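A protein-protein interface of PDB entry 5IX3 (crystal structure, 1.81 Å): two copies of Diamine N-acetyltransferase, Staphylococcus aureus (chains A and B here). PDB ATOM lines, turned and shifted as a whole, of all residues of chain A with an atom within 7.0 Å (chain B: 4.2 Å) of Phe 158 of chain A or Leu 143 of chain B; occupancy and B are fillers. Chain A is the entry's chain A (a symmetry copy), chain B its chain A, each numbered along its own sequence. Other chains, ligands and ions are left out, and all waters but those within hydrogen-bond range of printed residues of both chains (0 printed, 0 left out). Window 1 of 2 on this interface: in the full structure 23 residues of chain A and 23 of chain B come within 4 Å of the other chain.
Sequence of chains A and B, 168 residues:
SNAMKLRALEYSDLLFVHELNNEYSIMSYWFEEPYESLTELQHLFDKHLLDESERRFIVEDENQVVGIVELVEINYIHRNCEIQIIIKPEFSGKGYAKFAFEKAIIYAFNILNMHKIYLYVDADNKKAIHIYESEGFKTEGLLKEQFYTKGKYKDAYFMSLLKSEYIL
Phe 158 of chain A touches just one residue of chain B: Leu 143 (3.5 Å).
Of chain A, only Lys 116, Glu 140 and Phe 158 come within 4 Å of Leu 143 of chain B.
Printed residues of chain A within 4 Å of Gly 141 of chain B: Glu 140 and Gly 141.
Printed residues of chain A within 4 Å of Gln 146 of chain B: Lys 116 (2.6 Å) and Tyr 118 (3.8 Å).
Of the printed residues of chain A, Glu 145 of chain B touches Lys 116 (3.98 Å).
Lys 138 of chain A touches none of the printed residues of chain B.
The backbone NH (N) of Glu 140 of chain A lies within hydrogen-bond range of the backbone carbonyl oxygen (O) of Phe 158 of chain A (2.8 Å).
The backbone NH of Glu 145 of chain B is in hydrogen-bond range of the side-chain carboxylate of Asp 155 of chain B (2.8 Å).
The backbone carbonyl oxygen of Gly 141 of chain A sits at hydrogen-bond distance from the backbone NH of Phe 158 of chain A, at 2.9 Å.
The backbone NH (N) of Leu 143 of chain B is in hydrogen-bond range of the backbone carbonyl oxygen (O) of Ala 156 of chain B, at 2.7 Å.
The side-chain carboxylate (OE1) of Glu 140 of chain A sits close to the side-chain hydroxyl (OG) of Ser 160 of chain A, 3.1 Å away.
The side-chain amino group (NZ) of Lys 116 of chain A is in salt-bridge range of the side-chain carboxylate (OE1) of Glu 140 of chain A (2.7 Å).
Among the printed residues, pairs that only touch across the chains: Lys 116 of chain A with Leu 143 of chain B, Lys 116 of chain A with Glu 145 of chain B, Tyr 118 of chain A with Gln 146 of chain B, Glu 140 of chain A with Gly 141 of chain B, Glu 140 of chain A with Leu 143 of chain B, Gly 141 of chain A with Gly 141 of chain B and Phe 158 of chain A with Leu 143 of chain B.
Printed residues of chain B that touch a printed residue of chain A: Gly 141, Leu 142, Leu 143, Lys 144, Glu 145 and Gln 146.
Printed residues of chain A that touch a printed residue of chain B: Lys 116, Tyr 118, Glu 140, Gly 141 and Phe 158.
Hydrophobic or aromatic side chains of chain A within 4 Å of the printed part of chain B: Tyr 118 and Phe 158.
Among the printed residues, no Asp or Glu carboxylate lies within 4 Å of a Lys or Arg side-chain nitrogen of the other chain.
O of Lys 144 of chain B sits at hydrogen-bond distance from NZ of Lys 116 of chain A, 2.8 Å away.
O of Glu 140 of chain A sits at hydrogen-bond distance from N of Leu 142 of chain B, 2.9 Å away.
N of Lys 144 of chain B lies within hydrogen-bond range of OE2 of Glu 140 of chain A (2.8 Å).
OE1 of Gln 146 of chain B is in hydrogen-bond range of NZ of Lys 116 of chain A, at 2.6 Å.
Gly 141 of chain B touches its own counterpart, Gly 141 of chain A.
Of the 11 pairs that touch across the chains among the printed residues, 1 has its exchanged pair printed and touching as well.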
ATOM      1  N   LYS A 116      17.744  15.835 -13.512  1.00  0.00           N
ATOM      2  CA  LYS A 116      19.127  15.610 -12.969  1.00  0.00           C
ATOM      3  C   LYS A 116      19.778  14.475 -13.680  1.00  0.00           C
ATOM      4  O   LYS A 116      19.124  13.525 -14.133  1.00  0.00           O
ATOM      5  CB  LYS A 116      18.985  15.387 -11.482  1.00  0.00           C
ATOM      6  CG  LYS A 116      20.270  15.135 -10.699  1.00  0.00           C
ATOM      7  CD  LYS A 116      19.983  14.828  -9.277  1.00  0.00           C
ATOM      8  CE  LYS A 116      21.291  14.908  -8.495  1.00  0.00           C
ATOM      9  NZ  LYS A 116      21.211  14.397  -7.122  1.00  0.00           N
ATOM     10  N   ILE A 117      21.102  14.559 -13.880  1.00  0.00           N
ATOM     11  CA  ILE A 117      21.859  13.486 -14.375  1.00  0.00           C
ATOM     12  C   ILE A 117      22.994  13.225 -13.358  1.00  0.00           C
ATOM     13  O   ILE A 117      23.503  14.158 -12.775  1.00  0.00           O
ATOM     14  CB  ILE A 117      22.594  13.871 -15.694  1.00  0.00           C
ATOM     15  CG1 ILE A 117      21.645  14.453 -16.736  1.00  0.00           C
ATOM     16  CG2 ILE A 117      23.303  12.656 -16.214  1.00  0.00           C
ATOM     17  CD1 ILE A 117      20.563  13.520 -17.000  1.00  0.00           C
ATOM     18  N   TYR A 118      23.389  11.968 -13.223  1.00  0.00           N
ATOM     19  CA  TYR A 118      24.501  11.667 -12.269  1.00  0.00           C
ATOM     20  C   TYR A 118      25.377  10.605 -12.851  1.00  0.00           C
ATOM     21  O   TYR A 118      24.994   9.947 -13.813  1.00  0.00           O
ATOM     22  CB  TYR A 118      23.891  11.255 -10.906  1.00  0.00           C
ATOM     23  CG  TYR A 118      23.025  10.027 -10.935  1.00  0.00           C
ATOM     24  CD1 TYR A 118      21.639  10.129 -11.145  1.00  0.00           C
ATOM     25  CD2 TYR A 118      23.542   8.787 -10.792  1.00  0.00           C
ATOM     26  CE1 TYR A 118      20.865   9.016 -11.255  1.00  0.00           C
ATOM     27  CE2 TYR A 118      22.770   7.679 -10.839  1.00  0.00           C
ATOM     28  CZ  TYR A 118      21.434   7.776 -11.110  1.00  0.00           C
ATOM     29  OH  TYR A 118      20.677   6.646 -11.198  1.00  0.00           O
ATOM     30  N   LEU A 119      26.538  10.391 -12.226  1.00  0.00           N
ATOM     31  CA  LEU A 119      27.443   9.352 -12.676  1.00  0.00           C
ATOM     32  C   LEU A 119      28.226   8.886 -11.485  1.00  0.00           C
ATOM     33  O   LEU A 119      28.335   9.625 -10.483  1.00  0.00           O
ATOM     34  CB  LEU A 119      28.382   9.874 -13.785  1.00  0.00           C
ATOM     35  CG  LEU A 119      29.217  11.104 -13.555  1.00  0.00           C
ATOM     36  CD1 LEU A 119      30.505  10.688 -12.762  1.00  0.00           C
ATOM     37  CD2 LEU A 119      29.567  11.879 -14.781  1.00  0.00           C
ATOM     38  N   TYR A 120      28.842   7.737 -11.634  1.00  0.00           N
ATOM     39  CA  TYR A 120      29.876   7.274 -10.689  1.00  0.00           C
ATOM     40  C   TYR A 120      31.253   7.203 -11.385  1.00  0.00           C
ATOM     41  O   TYR A 120      31.368   6.905 -12.559  1.00  0.00           O
ATOM     42  CB  TYR A 120      29.545   5.873 -10.213  1.00  0.00           C
ATOM     43  CG  TYR A 120      28.207   5.703  -9.670  1.00  0.00           C
ATOM     44  CD1 TYR A 120      27.945   5.930  -8.352  1.00  0.00           C
ATOM     45  CD2 TYR A 120      27.146   5.292 -10.488  1.00  0.00           C
ATOM     46  CE1 TYR A 120      26.674   5.817  -7.836  1.00  0.00           C
ATOM     47  CE2 TYR A 120      25.872   5.146  -9.974  1.00  0.00           C
ATOM     48  CZ  TYR A 120      25.635   5.401  -8.669  1.00  0.00           C
ATOM     49  OH  TYR A 120      24.385   5.229  -8.178  1.00  0.00           O
ATOM     50  N   VAL A 121      32.308   7.526 -10.646  1.00  0.00           N
ATOM     51  CA  VAL A 121      33.629   7.560 -11.200  1.00  0.00           C
ATOM     52  C   VAL A 121      34.583   7.114 -10.066  1.00  0.00           C
ATOM     53  O   VAL A 121      34.436   7.505  -8.942  1.00  0.00           O
ATOM     54  CB  VAL A 121      33.986   8.916 -11.748  1.00  0.00           C
ATOM     55  CG1 VAL A 121      33.810  10.011 -10.714  1.00  0.00           C
ATOM     56  CG2 VAL A 121      35.329   8.909 -12.413  1.00  0.00           C
ATOM     57  N   LYS A 138      29.023  18.089 -10.243  1.00  0.00           N
ATOM     58  CA  LYS A 138      29.503  18.334  -8.907  1.00  0.00           C
ATOM     59  C   LYS A 138      29.532  17.085  -8.081  1.00  0.00           C
ATOM     60  O   LYS A 138      28.678  16.247  -8.201  1.00  0.00           O
ATOM     61  CB  LYS A 138      28.608  19.353  -8.246  1.00  0.00           C
ATOM     62  CG  LYS A 138      28.664  20.707  -9.010  1.00  0.00           C
ATOM     63  CD  LYS A 138      28.100  21.864  -8.167  1.00  0.00           C
ATOM     64  CE  LYS A 138      26.731  21.593  -7.562  1.00  0.00           C
ATOM     65  NZ  LYS A 138      26.352  22.726  -6.679  1.00  0.00           N
ATOM     66  N   THR A 139      30.537  16.926  -7.229  1.00  0.00           N
ATOM     67  CA  THR A 139      30.541  15.750  -6.339  1.00  0.00           C
ATOM     68  C   THR A 139      29.534  15.866  -5.215  1.00  0.00           C
ATOM     69  O   THR A 139      29.455  16.908  -4.554  1.00  0.00           O
ATOM     70  CB  THR A 139      31.927  15.567  -5.721  1.00  0.00           C
ATOM     71  OG1 THR A 139      32.794  15.454  -6.813  1.00  0.00           O
ATOM     72  CG2 THR A 139      31.980  14.327  -4.868  1.00  0.00           C
ATOM     73  N   GLU A 140      28.651  14.889  -5.117  1.00  0.00           N
ATOM     74  CA  GLU A 140      27.665  14.773  -4.020  1.00  0.00           C
ATOM     75  C   GLU A 140      27.916  13.694  -3.019  1.00  0.00           C
ATOM     76  O   GLU A 140      27.232  13.654  -1.980  1.00  0.00           O
ATOM     77  CB  GLU A 140      26.250  14.504  -4.603  1.00  0.00           C
ATOM     78  CG  GLU A 140      25.700  15.708  -5.355  1.00  0.00           C
ATOM     79  CD  GLU A 140      24.181  15.589  -5.650  1.00  0.00           C
ATOM     80  OE1 GLU A 140      23.701  14.515  -6.066  1.00  0.00           O
ATOM     81  OE2 GLU A 140      23.491  16.551  -5.409  1.00  0.00           O
ATOM     82  N   GLY A 141      28.872  12.815  -3.305  1.00  0.00           N
ATOM     83  CA  GLY A 141      29.132  11.717  -2.417  1.00  0.00           C
ATOM     84  C   GLY A 141      30.431  11.045  -2.726  1.00  0.00           C
ATOM     85  O   GLY A 141      30.924  11.114  -3.882  1.00  0.00           O
ATOM     86  N   LEU A 142      30.967  10.394  -1.688  1.00  0.00           N
ATOM     87  CA  LEU A 142      32.187   9.577  -1.810  1.00  0.00           C
ATOM     88  C   LEU A 142      31.849   8.231  -1.201  1.00  0.00           C
ATOM     89  O   LEU A 142      31.557   8.122   0.043  1.00  0.00           O
ATOM     90  CB  LEU A 142      33.395  10.248  -1.101  1.00  0.00           C
ATOM     91  CG  LEU A 142      34.637   9.341  -1.036  1.00  0.00           C
ATOM     92  CD1 LEU A 142      35.112   8.935  -2.382  1.00  0.00           C
ATOM     93  CD2 LEU A 142      35.723  10.176  -0.361  1.00  0.00           C
ATOM     94  N   LEU A 143      31.685   7.240  -2.105  1.00  0.00           N
ATOM     95  CA  LEU A 143      31.055   6.018  -1.711  1.00  0.00           C
ATOM     96  C   LEU A 143      32.224   5.048  -1.487  1.00  0.00           C
ATOM     97  O   LEU A 143      32.875   4.682  -2.438  1.00  0.00           O
ATOM     98  CB  LEU A 143      30.137   5.500  -2.818  1.00  0.00           C
ATOM     99  CG  LEU A 143      29.114   6.476  -3.341  1.00  0.00           C
ATOM    100  CD1 LEU A 143      28.284   5.766  -4.349  1.00  0.00           C
ATOM    101  CD2 LEU A 143      28.254   7.036  -2.243  1.00  0.00           C
ATOM    102  N   ALA A 156      34.249   5.484  -4.953  1.00  0.00           N
ATOM    103  CA  ALA A 156      33.732   6.152  -6.141  1.00  0.00           C
ATOM    104  C   ALA A 156      33.102   7.482  -5.726  1.00  0.00           C
ATOM    105  O   ALA A 156      32.439   7.562  -4.713  1.00  0.00           O
ATOM    106  CB  ALA A 156      32.681   5.319  -6.861  1.00  0.00           C
ATOM    107  N   TYR A 157      33.275   8.488  -6.554  1.00  0.00           N
ATOM    108  CA  TYR A 157      32.494   9.718  -6.400  1.00  0.00           C
ATOM    109  C   TYR A 157      31.175   9.536  -7.095  1.00  0.00           C
ATOM    110  O   TYR A 157      31.131   8.896  -8.053  1.00  0.00           O
ATOM    111  CB  TYR A 157      33.142  10.917  -6.946  1.00  0.00           C
ATOM    112  CG  TYR A 157      34.381  11.317  -6.252  1.00  0.00           C
ATOM    113  CD1 TYR A 157      34.340  11.653  -4.930  1.00  0.00           C
ATOM    114  CD2 TYR A 157      35.568  11.450  -6.944  1.00  0.00           C
ATOM    115  CE1 TYR A 157      35.457  12.087  -4.255  1.00  0.00           C
ATOM    116  CE2 TYR A 157      36.709  11.888  -6.260  1.00  0.00           C
ATOM    117  CZ  TYR A 157      36.616  12.198  -4.918  1.00  0.00           C
ATOM    118  OH  TYR A 157      37.715  12.602  -4.205  1.00  0.00           O
ATOM    119  N   PHE A 158      30.121   9.964  -6.462  1.00  0.00           N
ATOM    120  CA  PHE A 158      28.833  10.231  -7.085  1.00  0.00           C
ATOM    121  C   PHE A 158      28.834  11.689  -7.483  1.00  0.00           C
ATOM    122  O   PHE A 158      29.046  12.573  -6.646  1.00  0.00           O
ATOM    123  CB  PHE A 158      27.717   9.979  -6.010  1.00  0.00           C
ATOM    124  CG  PHE A 158      26.303  10.101  -6.550  1.00  0.00           C
ATOM    125  CD1 PHE A 158      25.732  11.294  -6.746  1.00  0.00           C
ATOM    126  CD2 PHE A 158      25.613   8.970  -6.860  1.00  0.00           C
ATOM    127  CE1 PHE A 158      24.481  11.367  -7.294  1.00  0.00           C
ATOM    128  CE2 PHE A 158      24.338   9.056  -7.378  1.00  0.00           C
ATOM    129  CZ  PHE A 158      23.792  10.241  -7.546  1.00  0.00           C
ATOM    130  N   MET A 159      28.699  11.960  -8.762  1.00  0.00           N
ATOM    131  CA  MET A 159      28.676  13.333  -9.258  1.00  0.00           C
ATOM    132  C   MET A 159      27.358  13.555  -9.970  1.00  0.00           C
ATOM    133  O   MET A 159      26.800  12.626 -10.603  1.00  0.00           O
ATOM    134  CB  MET A 159      29.869  13.554 -10.210  1.00  0.00           C
ATOM    135  CG  MET A 159      31.254  13.300  -9.517  1.00  0.00           C
ATOM    136  SD  MET A 159      32.585  13.639 -10.661  1.00  0.00           S
ATOM    137  CE  MET A 159      32.668  15.436 -10.477  1.00  0.00           C
ATOM    138  N   SER A 160      26.926  14.801 -10.025  1.00  0.00           N
ATOM    139  CA  SER A 160      25.633  15.081 -10.606  1.00  0.00           C
ATOM    140  C   SER A 160      25.547  16.446 -11.189  1.00  0.00           C
ATOM    141  O   SER A 160      26.314  17.345 -10.815  1.00  0.00           O
ATOM    142  CB  SER A 160      24.574  14.896  -9.479  1.00  0.00           C
ATOM    143  OG  SER A 160      24.578  15.997  -8.598  1.00  0.00           O
ATOM    144  N   TYR B 120      19.100   4.748   0.941  1.00  0.00           N
ATOM    145  CA  TYR B 120      18.749   6.170   0.754  1.00  0.00           C
ATOM    146  C   TYR B 120      17.614   6.579   1.718  1.00  0.00           C
ATOM    147  O   TYR B 120      16.734   5.805   2.044  1.00  0.00           O
ATOM    148  CB  TYR B 120      18.237   6.389  -0.656  1.00  0.00           C
ATOM    149  CG  TYR B 120      19.110   5.907  -1.714  1.00  0.00           C
ATOM    150  CD1 TYR B 120      20.096   6.695  -2.231  1.00  0.00           C
ATOM    151  CD2 TYR B 120      18.956   4.618  -2.241  1.00  0.00           C
ATOM    152  CE1 TYR B 120      20.957   6.233  -3.200  1.00  0.00           C
ATOM    153  CE2 TYR B 120      19.796   4.156  -3.237  1.00  0.00           C
ATOM    154  CZ  TYR B 120      20.780   4.948  -3.714  1.00  0.00           C
ATOM    155  OH  TYR B 120      21.578   4.487  -4.706  1.00  0.00           O
ATOM    156  N   GLY B 141      26.886  10.615   1.269  1.00  0.00           N
ATOM    157  CA  GLY B 141      26.486  11.517   0.226  1.00  0.00           C
ATOM    158  C   GLY B 141      25.194  12.200   0.544  1.00  0.00           C
ATOM    159  O   GLY B 141      24.371  11.668   1.334  1.00  0.00           O
ATOM    160  N   LEU B 142      25.028  13.368  -0.085  1.00  0.00           N
ATOM    161  CA  LEU B 142      23.780  14.145   0.006  1.00  0.00           C
ATOM    162  C   LEU B 142      23.378  14.456  -1.423  1.00  0.00           C
ATOM    163  O   LEU B 142      24.116  15.188  -2.173  1.00  0.00           O
ATOM    164  CB  LEU B 142      23.972  15.435   0.848  1.00  0.00           C
ATOM    165  CG  LEU B 142      22.751  16.373   0.807  1.00  0.00           C
ATOM    166  CD1 LEU B 142      21.519  15.719   1.314  1.00  0.00           C
ATOM    167  CD2 LEU B 142      23.100  17.545   1.720  1.00  0.00           C
ATOM    168  N   LEU B 143      22.323  13.740  -1.869  1.00  0.00           N
ATOM    169  CA  LEU B 143      22.043  13.688  -3.271  1.00  0.00           C
ATOM    170  C   LEU B 143      20.903  14.697  -3.463  1.00  0.00           C
ATOM    171  O   LEU B 143      19.814  14.451  -2.996  1.00  0.00           O
ATOM    172  CB  LEU B 143      21.591  12.287  -3.681  1.00  0.00           C
ATOM    173  CG  LEU B 143      22.501  11.154  -3.283  1.00  0.00           C
ATOM    174  CD1 LEU B 143      21.926   9.896  -3.831  1.00  0.00           C
ATOM    175  CD2 LEU B 143      23.905  11.356  -3.778  1.00  0.00           C
ATOM    176  N   LYS B 144      21.184  15.871  -3.997  1.00  0.00           N
ATOM    177  CA  LYS B 144      20.177  16.934  -3.984  1.00  0.00           C
ATOM    178  C   LYS B 144      19.135  16.745  -5.040  1.00  0.00           C
ATOM    179  O   LYS B 144      19.472  16.442  -6.168  1.00  0.00           O
ATOM    180  CB  LYS B 144      20.807  18.311  -4.115  1.00  0.00           C
ATOM    181  CG  LYS B 144      21.792  18.558  -2.921  1.00  0.00           C
ATOM    182  CD  LYS B 144      21.593  19.870  -2.193  1.00  0.00           C
ATOM    183  CE  LYS B 144      22.691  20.025  -1.120  1.00  0.00           C
ATOM    184  NZ  LYS B 144      22.952  21.435  -0.725  1.00  0.00           N
ATOM    185  N   GLU B 145      17.879  16.972  -4.668  1.00  0.00           N
ATOM    186  CA  GLU B 145      16.761  16.875  -5.675  1.00  0.00           C
ATOM    187  C   GLU B 145      16.743  15.536  -6.375  1.00  0.00           C
ATOM    188  O   GLU B 145      16.452  15.465  -7.553  1.00  0.00           O
ATOM    189  CB  GLU B 145      16.885  18.003  -6.703  1.00  0.00           C
ATOM    190  CG  GLU B 145      16.978  19.314  -5.962  1.00  0.00           C
ATOM    191  CD  GLU B 145      16.708  20.524  -6.776  1.00  0.00           C
ATOM    192  OE1 GLU B 145      17.207  21.569  -6.349  1.00  0.00           O
ATOM    193  OE2 GLU B 145      16.029  20.415  -7.788  1.00  0.00           O
ATOM    194  N   GLN B 146      17.086  14.488  -5.652  1.00  0.00           N
ATOM    195  CA  GLN B 146      17.195  13.182  -6.217  1.00  0.00           C
ATOM    196  C   GLN B 146      15.837  12.446  -6.382  1.00  0.00           C
ATOM    197  O   GLN B 146      15.739  11.503  -7.145  1.00  0.00           O
ATOM    198  CB  GLN B 146      18.103  12.343  -5.320  1.00  0.00           C
ATOM    199  CG  GLN B 146      18.463  10.997  -5.924  1.00  0.00           C
ATOM    200  CD  GLN B 146      19.436  11.084  -7.106  1.00  0.00           C
ATOM    201  OE1 GLN B 146      20.155  12.001  -7.260  1.00  0.00           O
ATOM    202  NE2 GLN B 146      19.410  10.087  -7.959  1.00  0.00           N
ATOM    203  N   ASP B 155      16.039  16.116  -1.256  1.00  0.00           N
ATOM    204  CA  ASP B 155      17.377  15.635  -1.113  1.00  0.00           C
ATOM    205  C   ASP B 155      17.364  14.346  -0.323  1.00  0.00           C
ATOM    206  O   ASP B 155      16.479  14.140   0.597  1.00  0.00           O
ATOM    207  CB  ASP B 155      18.148  16.687  -0.308  1.00  0.00           C
ATOM    208  CG  ASP B 155      18.209  18.037  -1.000  1.00  0.00           C
ATOM    209  OD1 ASP B 155      17.900  18.203  -2.202  1.00  0.00           O
ATOM    210  OD2 ASP B 155      18.654  18.972  -0.343  1.00  0.00           O
ATOM    211  N   ALA B 156      18.302  13.456  -0.633  1.00  0.00           N
ATOM    212  CA  ALA B 156      18.391  12.188   0.079  1.00  0.00           C
ATOM    213  C   ALA B 156      19.829  11.990   0.559  1.00  0.00           C
ATOM    214  O   ALA B 156      20.765  12.292  -0.151  1.00  0.00           O
ATOM    215  CB  ALA B 156      18.002  11.005  -0.795  1.00  0.00           C
